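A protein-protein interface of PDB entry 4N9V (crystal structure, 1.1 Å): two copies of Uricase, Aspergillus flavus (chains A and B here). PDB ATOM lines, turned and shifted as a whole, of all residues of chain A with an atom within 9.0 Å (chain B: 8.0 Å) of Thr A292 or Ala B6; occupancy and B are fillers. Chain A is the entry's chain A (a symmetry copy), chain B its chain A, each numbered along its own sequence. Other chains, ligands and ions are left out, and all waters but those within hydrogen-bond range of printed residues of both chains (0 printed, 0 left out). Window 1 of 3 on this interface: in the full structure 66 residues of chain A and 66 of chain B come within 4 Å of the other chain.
The backbone NH (N) of Thr A292 lies within hydrogen-bond range of the backbone carbonyl oxygen (O) of Ala B6, at 2.8 Å. The backbone carbonyl oxygen (O) of Gly A294 lies within hydrogen-bond range of the backbone NH (N) of Ala B3 (2.9 Å). N of Lys B5 sits at hydrogen-bond distance from O of Thr A292, at 2.8 Å. N of Lys A290 is in hydrogen-bond range of O of Arg B8, at 2.9 Å. OH of Tyr B47 sits at hydrogen-bond distance from O of Lys A290 (2.8 Å). NZ of Lys B5 sits at hydrogen-bond distance from O of Arg A295, 2.9 Å away. OH of Tyr A233 sits at hydrogen-bond distance from N of Ala B3 (3.5 Å).
Of the 11 printed residues of chain B, 7 touch a printed residue of chain A. Hydrophobic or aromatic side chains of chain B within 4 Å of the printed part of chain A: Val B4, Ala B7 and Tyr B47. Of the 22 printed residues of chain A, 9 touch a printed residue of chain B. Hydrophobic or aromatic side chains of chain A within 4 Å of the printed part of chain B: Met A232, Tyr A233, Ile A289 and Val A293. Along chain A the printed residues that touch a printed residue of chain B span positions 232 to 295. Among the printed residues, 18 pairs touch across the chains. Among the printed residues, no Asp or Glu carboxylate lies within 4 Å of a Lys or Arg side-chain nitrogen of the other chain.
No position is printed for both chains. Of the 18 pairs that touch across the chains among the printed residues, none has its exchanged pair printed and touching as well.
N of Tyr A251 is in hydrogen-bond range of O of Cys A291 (2.9 Å). OE2 of Glu A250 is in salt-bridge range of NZ of Lys A290 (3.8 Å). The backbone NH (N) of Val A293 is in hydrogen-bond range of the backbone carbonyl oxygen (O) of Val A249 (2.8 Å). The guanidinium group (NH2) of Arg B8 lies within salt-bridge range of the side-chain carboxylate (OE2) of Glu B40 (3.6 Å). O of Leu A240 sits at hydrogen-bond distance from NH2 of Arg A295 (2.9 Å).
Lys A144 touches none of the printed residues of chain B. Printed residues of chain B within 4 Å of Tyr A233: Ala B3 (3.5 Å), Val B4 (3.7 Å) and Tyr B47 (3.3 Å). Of the printed residues of chain B, Thr A292 touches Val B4, Lys B5 and Ala B6. Of the printed residues of chain A, Ala B6 touches Cys A291 (3.4 Å) and Thr A292 (2.8 Å). Of the printed residues of chain A, Tyr B47 touches Met A232, Tyr A233, Ile A289, Lys A290 and Cys A291. The nearest residue of chain B that does not touch Thr A292 is Ala B3 (4.2 Å).
Among the printed residues, pairs that only touch across the chains: Met A232 with Tyr B47, Tyr A233 with Val B4, Tyr A233 with Tyr B47, Ile A289 with Arg B8, Ile A289 with Tyr B47, Lys A290 with Ala B7, Cys A291 with Ala B6, Cys A291 with Tyr B47, Thr A292 with Val B4, Val A293 with Ala B3 and Gly A294 with Lys B5.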
ATOM      1  N   LYS A 144      24.664  41.294  30.365  1.00  0.00           N
ATOM      2  CA  LYS A 144      24.975  39.892  30.585  1.00  0.00           C
ATOM      3  C   LYS A 144      25.626  39.767  31.958  1.00  0.00           C
ATOM      4  O   LYS A 144      26.700  40.314  32.204  1.00  0.00           O
ATOM      5  CB  LYS A 144      25.937  39.383  29.524  1.00  0.00           C
ATOM      6  CG  LYS A 144      25.322  39.298  28.152  1.00  0.00           C
ATOM      7  CD  LYS A 144      26.382  39.125  27.074  1.00  0.00           C
ATOM      8  CE  LYS A 144      27.064  37.787  27.200  1.00  0.00           C
ATOM      9  N   THR A 186      26.356  32.427  32.437  1.00  0.00           N
ATOM     10  CA  THR A 186      25.923  33.770  32.051  1.00  0.00           C
ATOM     11  C   THR A 186      24.424  33.796  31.807  1.00  0.00           C
ATOM     12  O   THR A 186      23.891  32.951  31.086  1.00  0.00           O
ATOM     13  CB  THR A 186      26.623  34.206  30.759  1.00  0.00           C
ATOM     14  OG1 THR A 186      28.028  34.235  30.970  1.00  0.00           O
ATOM     15  CG2 THR A 186      26.173  35.582  30.314  1.00  0.00           C
ATOM     16  N   TRP A 187      23.739  34.774  32.391  1.00  0.00           N
ATOM     17  CA  TRP A 187      22.336  35.019  32.083  1.00  0.00           C
ATOM     18  C   TRP A 187      22.212  36.376  31.400  1.00  0.00           C
ATOM     19  O   TRP A 187      22.742  37.384  31.863  1.00  0.00           O
ATOM     20  CB  TRP A 187      21.435  34.864  33.322  1.00  0.00           C
ATOM     21  CG  TRP A 187      21.919  35.511  34.591  1.00  0.00           C
ATOM     22  CD1 TRP A 187      21.417  36.630  35.185  1.00  0.00           C
ATOM     23  CD2 TRP A 187      22.967  35.040  35.452  1.00  0.00           C
ATOM     24  NE1 TRP A 187      22.086  36.899  36.347  1.00  0.00           N
ATOM     25  CE2 TRP A 187      23.059  35.949  36.525  1.00  0.00           C
ATOM     26  CE3 TRP A 187      23.857  33.957  35.409  1.00  0.00           C
ATOM     27  CZ2 TRP A 187      24.009  35.811  37.540  1.00  0.00           C
ATOM     28  CZ3 TRP A 187      24.800  33.828  36.426  1.00  0.00           C
ATOM     29  CH2 TRP A 187      24.867  34.751  37.467  1.00  0.00           C
ATOM     30  N   GLN A 188      21.537  36.353  30.258  1.00  0.00           N
ATOM     31  CA  GLN A 188      21.341  37.529  29.405  1.00  0.00           C
ATOM     32  C   GLN A 188      19.975  38.116  29.674  1.00  0.00           C
ATOM     33  O   GLN A 188      18.965  37.449  29.470  1.00  0.00           O
ATOM     34  CB  GLN A 188      21.431  37.152  27.917  1.00  0.00           C
ATOM     35  CG  GLN A 188      20.862  38.193  26.950  1.00  0.00           C
ATOM     36  CD  GLN A 188      21.768  39.391  26.757  1.00  0.00           C
ATOM     37  OE1 GLN A 188      21.450  40.513  27.166  1.00  0.00           O
ATOM     38  NE2 GLN A 188      22.892  39.169  26.110  1.00  0.00           N
ATOM     39  N   MET A 232      24.401  20.369  32.592  1.00  0.00           N
ATOM     40  CA  MET A 232      24.386  21.814  32.425  1.00  0.00           C
ATOM     41  C   MET A 232      23.038  22.269  31.844  1.00  0.00           C
ATOM     42  O   MET A 232      22.539  23.339  32.176  1.00  0.00           O
ATOM     43  CB  MET A 232      25.557  22.275  31.553  1.00  0.00           C
ATOM     44  CG  MET A 232      25.457  21.881  30.094  1.00  0.00           C
ATOM     45  SD  MET A 232      27.044  21.835  29.236  1.00  0.00           S
ATOM     46  CE  MET A 232      27.576  23.528  29.416  1.00  0.00           C
ATOM     47  N   TYR A 233      22.437  21.463  30.975  1.00  0.00           N
ATOM     48  CA  TYR A 233      21.157  21.830  30.399  1.00  0.00           C
ATOM     49  C   TYR A 233      20.109  21.941  31.510  1.00  0.00           C
ATOM     50  O   TYR A 233      19.279  22.853  31.514  1.00  0.00           O
ATOM     51  CB  TYR A 233      20.731  20.816  29.331  1.00  0.00           C
ATOM     52  CG  TYR A 233      19.440  21.225  28.665  1.00  0.00           C
ATOM     53  CD1 TYR A 233      19.436  22.177  27.667  1.00  0.00           C
ATOM     54  CD2 TYR A 233      18.222  20.692  29.068  1.00  0.00           C
ATOM     55  CE1 TYR A 233      18.256  22.596  27.073  1.00  0.00           C
ATOM     56  CE2 TYR A 233      17.032  21.102  28.475  1.00  0.00           C
ATOM     57  CZ  TYR A 233      17.074  22.056  27.476  1.00  0.00           C
ATOM     58  OH  TYR A 233      15.929  22.498  26.851  1.00  0.00           O
ATOM     59  N   ALA A 236      20.440  25.246  33.294  1.00  0.00           N
ATOM     60  CA  ALA A 236      19.968  26.373  32.500  1.00  0.00           C
ATOM     61  C   ALA A 236      18.446  26.436  32.470  1.00  0.00           C
ATOM     62  O   ALA A 236      17.848  27.513  32.618  1.00  0.00           O
ATOM     63  CB  ALA A 236      20.529  26.286  31.093  1.00  0.00           C
ATOM     64  N   GLU A 237      17.796  25.286  32.289  1.00  0.00           N
ATOM     65  CA  GLU A 237      16.345  25.284  32.186  1.00  0.00           C
ATOM     66  C   GLU A 237      15.705  25.750  33.499  1.00  0.00           C
ATOM     67  O   GLU A 237      14.730  26.500  33.481  1.00  0.00           O
ATOM     68  CB  GLU A 237      15.826  23.930  31.678  1.00  0.00           C
ATOM     69  CG  GLU A 237      15.793  22.785  32.628  1.00  0.00           C
ATOM     70  CD  GLU A 237      15.412  21.473  31.917  1.00  0.00           C
ATOM     71  OE1 GLU A 237      14.497  21.467  31.041  1.00  0.00           O
ATOM     72  OE2 GLU A 237      16.033  20.437  32.239  1.00  0.00           O
ATOM     73  N   LEU A 240      16.083  29.666  33.824  1.00  0.00           N
ATOM     74  CA  LEU A 240      15.099  30.334  32.972  1.00  0.00           C
ATOM     75  C   LEU A 240      13.707  30.273  33.579  1.00  0.00           C
ATOM     76  O   LEU A 240      12.944  31.229  33.496  1.00  0.00           O
ATOM     77  CB  LEU A 240      15.084  29.714  31.584  1.00  0.00           C
ATOM     78  CG  LEU A 240      16.277  30.043  30.692  1.00  0.00           C
ATOM     79  CD1 LEU A 240      16.282  29.152  29.458  1.00  0.00           C
ATOM     80  CD2 LEU A 240      16.300  31.516  30.290  1.00  0.00           C
ATOM     81  N   GLU A 247      16.541  36.137  29.091  1.00  0.00           N
ATOM     82  CA  GLU A 247      16.222  35.525  27.811  1.00  0.00           C
ATOM     83  C   GLU A 247      16.989  34.241  27.530  1.00  0.00           C
ATOM     84  O   GLU A 247      16.437  33.324  26.932  1.00  0.00           O
ATOM     85  CB  GLU A 247      16.481  36.529  26.692  1.00  0.00           C
ATOM     86  CG  GLU A 247      15.520  37.728  26.772  1.00  0.00           C
ATOM     87  CD  GLU A 247      15.677  38.747  25.653  1.00  0.00           C
ATOM     88  OE1 GLU A 247      16.713  38.742  24.963  1.00  0.00           O
ATOM     89  OE2 GLU A 247      14.749  39.565  25.475  1.00  0.00           O
ATOM     90  N   THR A 248      18.259  34.188  27.933  1.00  0.00           N
ATOM     91  CA  THR A 248      19.072  33.002  27.730  1.00  0.00           C
ATOM     92  C   THR A 248      19.985  32.783  28.919  1.00  0.00           C
ATOM     93  O   THR A 248      20.317  33.712  29.669  1.00  0.00           O
ATOM     94  CB  THR A 248      19.942  33.081  26.461  1.00  0.00           C
ATOM     95  OG1 THR A 248      20.873  34.156  26.564  1.00  0.00           O
ATOM     96  CG2 THR A 248      19.097  33.269  25.214  1.00  0.00           C
ATOM     97  N   VAL A 249      20.387  31.529  29.071  1.00  0.00           N
ATOM     98  CA  VAL A 249      21.426  31.126  30.009  1.00  0.00           C
ATOM     99  C   VAL A 249      22.469  30.335  29.246  1.00  0.00           C
ATOM    100  O   VAL A 249      22.140  29.431  28.497  1.00  0.00           O
ATOM    101  CB  VAL A 249      20.848  30.280  31.159  1.00  0.00           C
ATOM    102  CG1 VAL A 249      21.960  29.773  32.075  1.00  0.00           C
ATOM    103  CG2 VAL A 249      19.819  31.070  31.936  1.00  0.00           C
ATOM    104  N   GLU A 250      23.727  30.685  29.456  1.00  0.00           N
ATOM    105  CA  GLU A 250      24.849  30.056  28.783  1.00  0.00           C
ATOM    106  C   GLU A 250      25.781  29.479  29.817  1.00  0.00           C
ATOM    107  O   GLU A 250      26.115  30.154  30.787  1.00  0.00           O
ATOM    108  CB  GLU A 250      25.625  31.095  27.980  1.00  0.00           C
ATOM    109  CG  GLU A 250      26.749  30.543  27.147  1.00  0.00           C
ATOM    110  CD  GLU A 250      27.619  31.638  26.529  1.00  0.00           C
ATOM    111  OE1 GLU A 250      27.266  32.839  26.605  1.00  0.00           O
ATOM    112  OE2 GLU A 250      28.676  31.296  25.971  1.00  0.00           O
ATOM    113  N   TYR A 251      26.227  28.251  29.600  1.00  0.00           N
ATOM    114  CA  TYR A 251      27.274  27.642  30.416  1.00  0.00           C
ATOM    115  C   TYR A 251      28.463  27.316  29.548  1.00  0.00           C
ATOM    116  O   TYR A 251      28.316  26.900  28.393  1.00  0.00           O
ATOM    117  CB  TYR A 251      26.783  26.353  31.086  1.00  0.00           C
ATOM    118  CG  TYR A 251      26.013  26.561  32.370  1.00  0.00           C
ATOM    119  CD1 TYR A 251      26.648  26.497  33.599  1.00  0.00           C
ATOM    120  CD2 TYR A 251      24.649  26.814  32.358  1.00  0.00           C
ATOM    121  CE1 TYR A 251      25.955  26.691  34.768  1.00  0.00           C
ATOM    122  CE2 TYR A 251      23.947  27.001  33.521  1.00  0.00           C
ATOM    123  CZ  TYR A 251      24.603  26.959  34.723  1.00  0.00           C
ATOM    124  OH  TYR A 251      23.879  27.156  35.861  1.00  0.00           O
ATOM    125  N   SER A 252      29.645  27.481  30.136  1.00  0.00           N
ATOM    126  CA  SER A 252      30.882  27.013  29.555  1.00  0.00           C
ATOM    127  C   SER A 252      31.621  26.279  30.649  1.00  0.00           C
ATOM    128  O   SER A 252      32.009  26.885  31.645  1.00  0.00           O
ATOM    129  CB  SER A 252      31.693  28.187  29.044  1.00  0.00           C
ATOM    130  OG  SER A 252      32.879  27.746  28.456  1.00  0.00           O
ATOM    131  N   ILE A 289      32.761  22.077  27.274  1.00  0.00           N
ATOM    132  CA  ILE A 289      31.380  21.811  26.901  1.00  0.00           C
ATOM    133  C   ILE A 289      30.608  23.117  27.052  1.00  0.00           C
ATOM    134  O   ILE A 289      30.677  23.757  28.100  1.00  0.00           O
ATOM    135  CB  ILE A 289      30.758  20.714  27.814  1.00  0.00           C
ATOM    136  CG1 ILE A 289      31.737  19.538  28.057  1.00  0.00           C
ATOM    137  CG2 ILE A 289      29.416  20.268  27.269  1.00  0.00           C
ATOM    138  CD1 ILE A 289      32.193  18.755  26.844  1.00  0.00           C
ATOM    139  N   LYS A 290      29.878  23.512  26.010  1.00  0.00           N
ATOM    140  CA  LYS A 290      29.182  24.790  25.997  1.00  0.00           C
ATOM    141  C   LYS A 290      27.745  24.628  25.529  1.00  0.00           C
ATOM    142  O   LYS A 290      27.439  23.803  24.655  1.00  0.00           O
ATOM    143  CB  LYS A 290      29.891  25.777  25.065  1.00  0.00           C
ATOM    144  CG  LYS A 290      31.306  26.106  25.507  1.00  0.00           C
ATOM    145  CD  LYS A 290      32.178  26.717  24.436  1.00  0.00           C
ATOM    146  CE  LYS A 290      31.616  27.977  23.875  1.00  0.00           C
ATOM    147  NZ  LYS A 290      31.565  29.036  24.897  1.00  0.00           N
ATOM    148  N   CYS A 291      26.856  25.435  26.081  1.00  0.00           N
ATOM    149  CA  CYS A 291      25.460  25.462  25.642  1.00  0.00           C
ATOM    150  C   CYS A 291      24.896  26.852  25.923  1.00  0.00           C
ATOM    151  O   CYS A 291      25.202  27.423  26.970  1.00  0.00           O
ATOM    152  CB  CYS A 291      24.669  24.407  26.432  1.00  0.00           C
ATOM    153  SG  CYS A 291      23.032  23.938  25.795  1.00  0.00           S
ATOM    154  N   THR A 292      24.035  27.329  25.043  1.00  0.00           N
ATOM    155  CA  THR A 292      23.181  28.472  25.287  1.00  0.00           C
ATOM    156  C   THR A 292      21.754  27.982  25.172  1.00  0.00           C
ATOM    157  O   THR A 292      21.357  27.406  24.163  1.00  0.00           O
ATOM    158  CB  THR A 292      23.416  29.593  24.286  1.00  0.00           C
ATOM    159  OG1 THR A 292      24.792  29.964  24.338  1.00  0.00           O
ATOM    160  CG2 THR A 292      22.529  30.821  24.603  1.00  0.00           C
ATOM    161  N   VAL A 293      20.995  28.198  26.230  1.00  0.00           N
ATOM    162  CA  VAL A 293      19.618  27.756  26.313  1.00  0.00           C
ATOM    163  C   VAL A 293      18.714  28.971  26.377  1.00  0.00           C
ATOM    164  O   VAL A 293      18.969  29.938  27.092  1.00  0.00           O
ATOM    165  CB  VAL A 293      19.421  26.874  27.565  1.00  0.00           C
ATOM    166  CG1 VAL A 293      18.007  26.353  27.666  1.00  0.00           C
ATOM    167  CG2 VAL A 293      20.420  25.715  27.560  1.00  0.00           C
ATOM    168  N   GLY A 294      17.648  28.912  25.589  1.00  0.00           N
ATOM    169  CA  GLY A 294      16.666  29.964  25.549  1.00  0.00           C
ATOM    170  C   GLY A 294      15.304  29.355  25.726  1.00  0.00           C
ATOM    171  O   GLY A 294      15.158  28.176  26.029  1.00  0.00           O
ATOM    172  N   ARG A 295      14.294  30.187  25.541  1.00  0.00           N
ATOM    173  CA  ARG A 295      12.920  29.775  25.766  1.00  0.00           C
ATOM    174  C   ARG A 295      12.338  29.199  24.484  1.00  0.00           C
ATOM    175  O   ARG A 295      12.629  29.683  23.394  1.00  0.00           O
ATOM    176  CB  ARG A 295      12.107  30.975  26.256  1.00  0.00           C
ATOM    177  CG  ARG A 295      12.771  31.675  27.439  1.00  0.00           C
ATOM    178  CD  ARG A 295      12.020  32.915  27.920  1.00  0.00           C
ATOM    179  NE  ARG A 295      12.604  33.418  29.165  1.00  0.00           N
ATOM    180  CZ  ARG A 295      12.476  32.800  30.332  1.00  0.00           C
ATOM    181  NH1 ARG A 295      11.794  31.664  30.410  1.00  0.00           N
ATOM    182  NH2 ARG A 295      13.040  33.290  31.423  1.00  0.00           N
ATOM    183  N   ALA B   3      14.862  25.377  25.219  1.00  0.00           N
ATOM    184  CA  ALA B   3      15.459  24.732  24.066  1.00  0.00           C
ATOM    185  C   ALA B   3      16.909  25.181  23.894  1.00  0.00           C
ATOM    186  O   ALA B   3      17.302  26.292  24.289  1.00  0.00           O
ATOM    187  CB  ALA B   3      14.658  25.044  22.806  1.00  0.00           C
ATOM    188  N   VAL B   4      17.700  24.312  23.284  1.00  0.00           N
ATOM    189  CA  VAL B   4      19.070  24.655  22.953  1.00  0.00           C
ATOM    190  C   VAL B   4      19.089  25.661  21.807  1.00  0.00           C
ATOM    191  O   VAL B   4      18.547  25.397  20.742  1.00  0.00           O
ATOM    192  CB  VAL B   4      19.860  23.404  22.566  1.00  0.00           C
ATOM    193  CG1 VAL B   4      21.246  23.782  22.087  1.00  0.00           C
ATOM    194  CG2 VAL B   4      19.942  22.433  23.747  1.00  0.00           C
ATOM    195  N   LYS B   5      19.688  26.818  22.041  1.00  0.00           N
ATOM    196  CA  LYS B   5      19.869  27.824  21.007  1.00  0.00           C
ATOM    197  C   LYS B   5      21.227  27.709  20.321  1.00  0.00           C
ATOM    198  O   LYS B   5      21.364  28.020  19.137  1.00  0.00           O
ATOM    199  CB  LYS B   5      19.700  29.217  21.615  1.00  0.00           C
ATOM    200  CG  LYS B   5      18.304  29.448  22.212  1.00  0.00           C
ATOM    201  CD  LYS B   5      17.183  29.223  21.184  1.00  0.00           C
ATOM    202  CE  LYS B   5      15.831  28.995  21.859  1.00  0.00           C
ATOM    203  NZ  LYS B   5      15.271  30.216  22.460  1.00  0.00           N
ATOM    204  N   ALA B   6      22.230  27.258  21.073  1.00  0.00           N
ATOM    205  CA  ALA B   6      23.569  27.053  20.539  1.00  0.00           C
ATOM    206  C   ALA B   6      24.238  25.993  21.387  1.00  0.00           C
ATOM    207  O   ALA B   6      23.970  25.897  22.583  1.00  0.00           O
ATOM    208  CB  ALA B   6      24.368  28.334  20.586  1.00  0.00           C
ATOM    209  N   ALA B   7      25.110  25.207  20.776  1.00  0.00           N
ATOM    210  CA  ALA B   7      25.879  24.221  21.509  1.00  0.00           C
ATOM    211  C   ALA B   7      27.136  23.894  20.746  1.00  0.00           C
ATOM    212  O   ALA B   7      27.124  23.745  19.517  1.00  0.00           O
ATOM    213  CB  ALA B   7      25.063  22.984  21.721  1.00  0.00           C
ATOM    214  N   ARG B   8      28.230  23.766  21.489  1.00  0.00           N
ATOM    215  CA  ARG B   8      29.465  23.270  20.926  1.00  0.00           C
ATOM    216  C   ARG B   8      30.252  22.608  22.029  1.00  0.00           C
ATOM    217  O   ARG B   8      30.092  22.944  23.201  1.00  0.00           O
ATOM    218  CB  ARG B   8      30.277  24.354  20.220  1.00  0.00           C
ATOM    219  CG  ARG B   8      30.820  25.437  21.093  1.00  0.00           C
ATOM    220  CD  ARG B   8      31.633  26.434  20.277  1.00  0.00           C
ATOM    221  NE  ARG B   8      30.800  27.113  19.289  1.00  0.00           N
ATOM    222  CZ  ARG B   8      31.244  28.029  18.435  1.00  0.00           C
ATOM    223  NH1 ARG B   8      32.522  28.378  18.449  1.00  0.00           N
ATOM    224  NH2 ARG B   8      30.409  28.599  17.570  1.00  0.00           N
ATOM    225  N   GLU B  40      30.153  21.391  16.370  1.00  0.00           N
ATOM    226  CA  GLU B  40      28.731  21.702  16.366  1.00  0.00           C
ATOM    227  C   GLU B  40      28.017  20.790  15.387  1.00  0.00           C
ATOM    228  O   GLU B  40      28.598  20.336  14.407  1.00  0.00           O
ATOM    229  CB  GLU B  40      28.460  23.117  15.866  1.00  0.00           C
ATOM    230  CG  GLU B  40      28.977  24.248  16.693  1.00  0.00           C
ATOM    231  CD  GLU B  40      28.459  25.549  16.113  1.00  0.00           C
ATOM    232  OE1 GLU B  40      27.310  25.923  16.404  1.00  0.00           O
ATOM    233  OE2 GLU B  40      29.162  26.163  15.293  1.00  0.00           O
ATOM    234  N   GLY B  41      26.731  20.575  15.614  1.00  0.00           N
ATOM    235  CA  GLY B  41      25.924  19.862  14.649  1.00  0.00           C
ATOM    236  C   GLY B  41      24.646  19.410  15.298  1.00  0.00           C
ATOM    237  O   GLY B  41      24.113  20.088  16.170  1.00  0.00           O
ATOM    238  N   ILE B  43      23.514  17.728  17.703  1.00  0.00           N
ATOM    239  CA  ILE B  43      23.985  17.189  18.972  1.00  0.00           C
ATOM    240  C   ILE B  43      23.106  17.613  20.140  1.00  0.00           C
ATOM    241  O   ILE B  43      23.398  17.298  21.285  1.00  0.00           O
ATOM    242  CB  ILE B  43      25.460  17.608  19.259  1.00  0.00           C
ATOM    243  CG1 ILE B  43      25.595  19.138  19.324  1.00  0.00           C
ATOM    244  CG2 ILE B  43      26.385  17.006  18.209  1.00  0.00           C
ATOM    245  CD1 ILE B  43      26.941  19.619  19.840  1.00  0.00           C
ATOM    246  N   GLU B  44      22.034  18.345  19.876  1.00  0.00           N
ATOM    247  CA  GLU B  44      21.254  18.905  20.972  1.00  0.00           C
ATOM    248  C   GLU B  44      20.691  17.850  21.914  1.00  0.00           C
ATOM    249  O   GLU B  44      20.525  18.122  23.105  1.00  0.00           O
ATOM    250  CB  GLU B  44      20.108  19.793  20.468  1.00  0.00           C
ATOM    251  CG  GLU B  44      20.456  20.668  19.297  1.00  0.00           C
ATOM    252  CD  GLU B  44      20.607  19.858  18.028  1.00  0.00           C
ATOM    253  OE1 GLU B  44      19.854  18.883  17.858  1.00  0.00           O
ATOM    254  OE2 GLU B  44      21.489  20.165  17.221  1.00  0.00           O
ATOM    255  N   TYR B  47      22.282  17.123  25.212  1.00  0.00           N
ATOM    256  CA  TYR B  47      21.934  18.062  26.269  1.00  0.00           C
ATOM    257  C   TYR B  47      20.525  17.825  26.807  1.00  0.00           C
ATOM    258  O   TYR B  47      20.298  17.874  28.016  1.00  0.00           O
ATOM    259  CB  TYR B  47      22.044  19.505  25.768  1.00  0.00           C
ATOM    260  CG  TYR B  47      23.436  19.908  25.319  1.00  0.00           C
ATOM    261  CD1 TYR B  47      23.907  19.587  24.057  1.00  0.00           C
ATOM    262  CD2 TYR B  47      24.280  20.619  26.165  1.00  0.00           C
ATOM    263  CE1 TYR B  47      25.162  19.969  23.630  1.00  0.00           C
ATOM    264  CE2 TYR B  47      25.539  21.000  25.747  1.00  0.00           C
ATOM    265  CZ  TYR B  47      25.979  20.687  24.482  1.00  0.00           C
ATOM    266  OH  TYR B  47      27.227  21.060  24.039  1.00  0.00           O
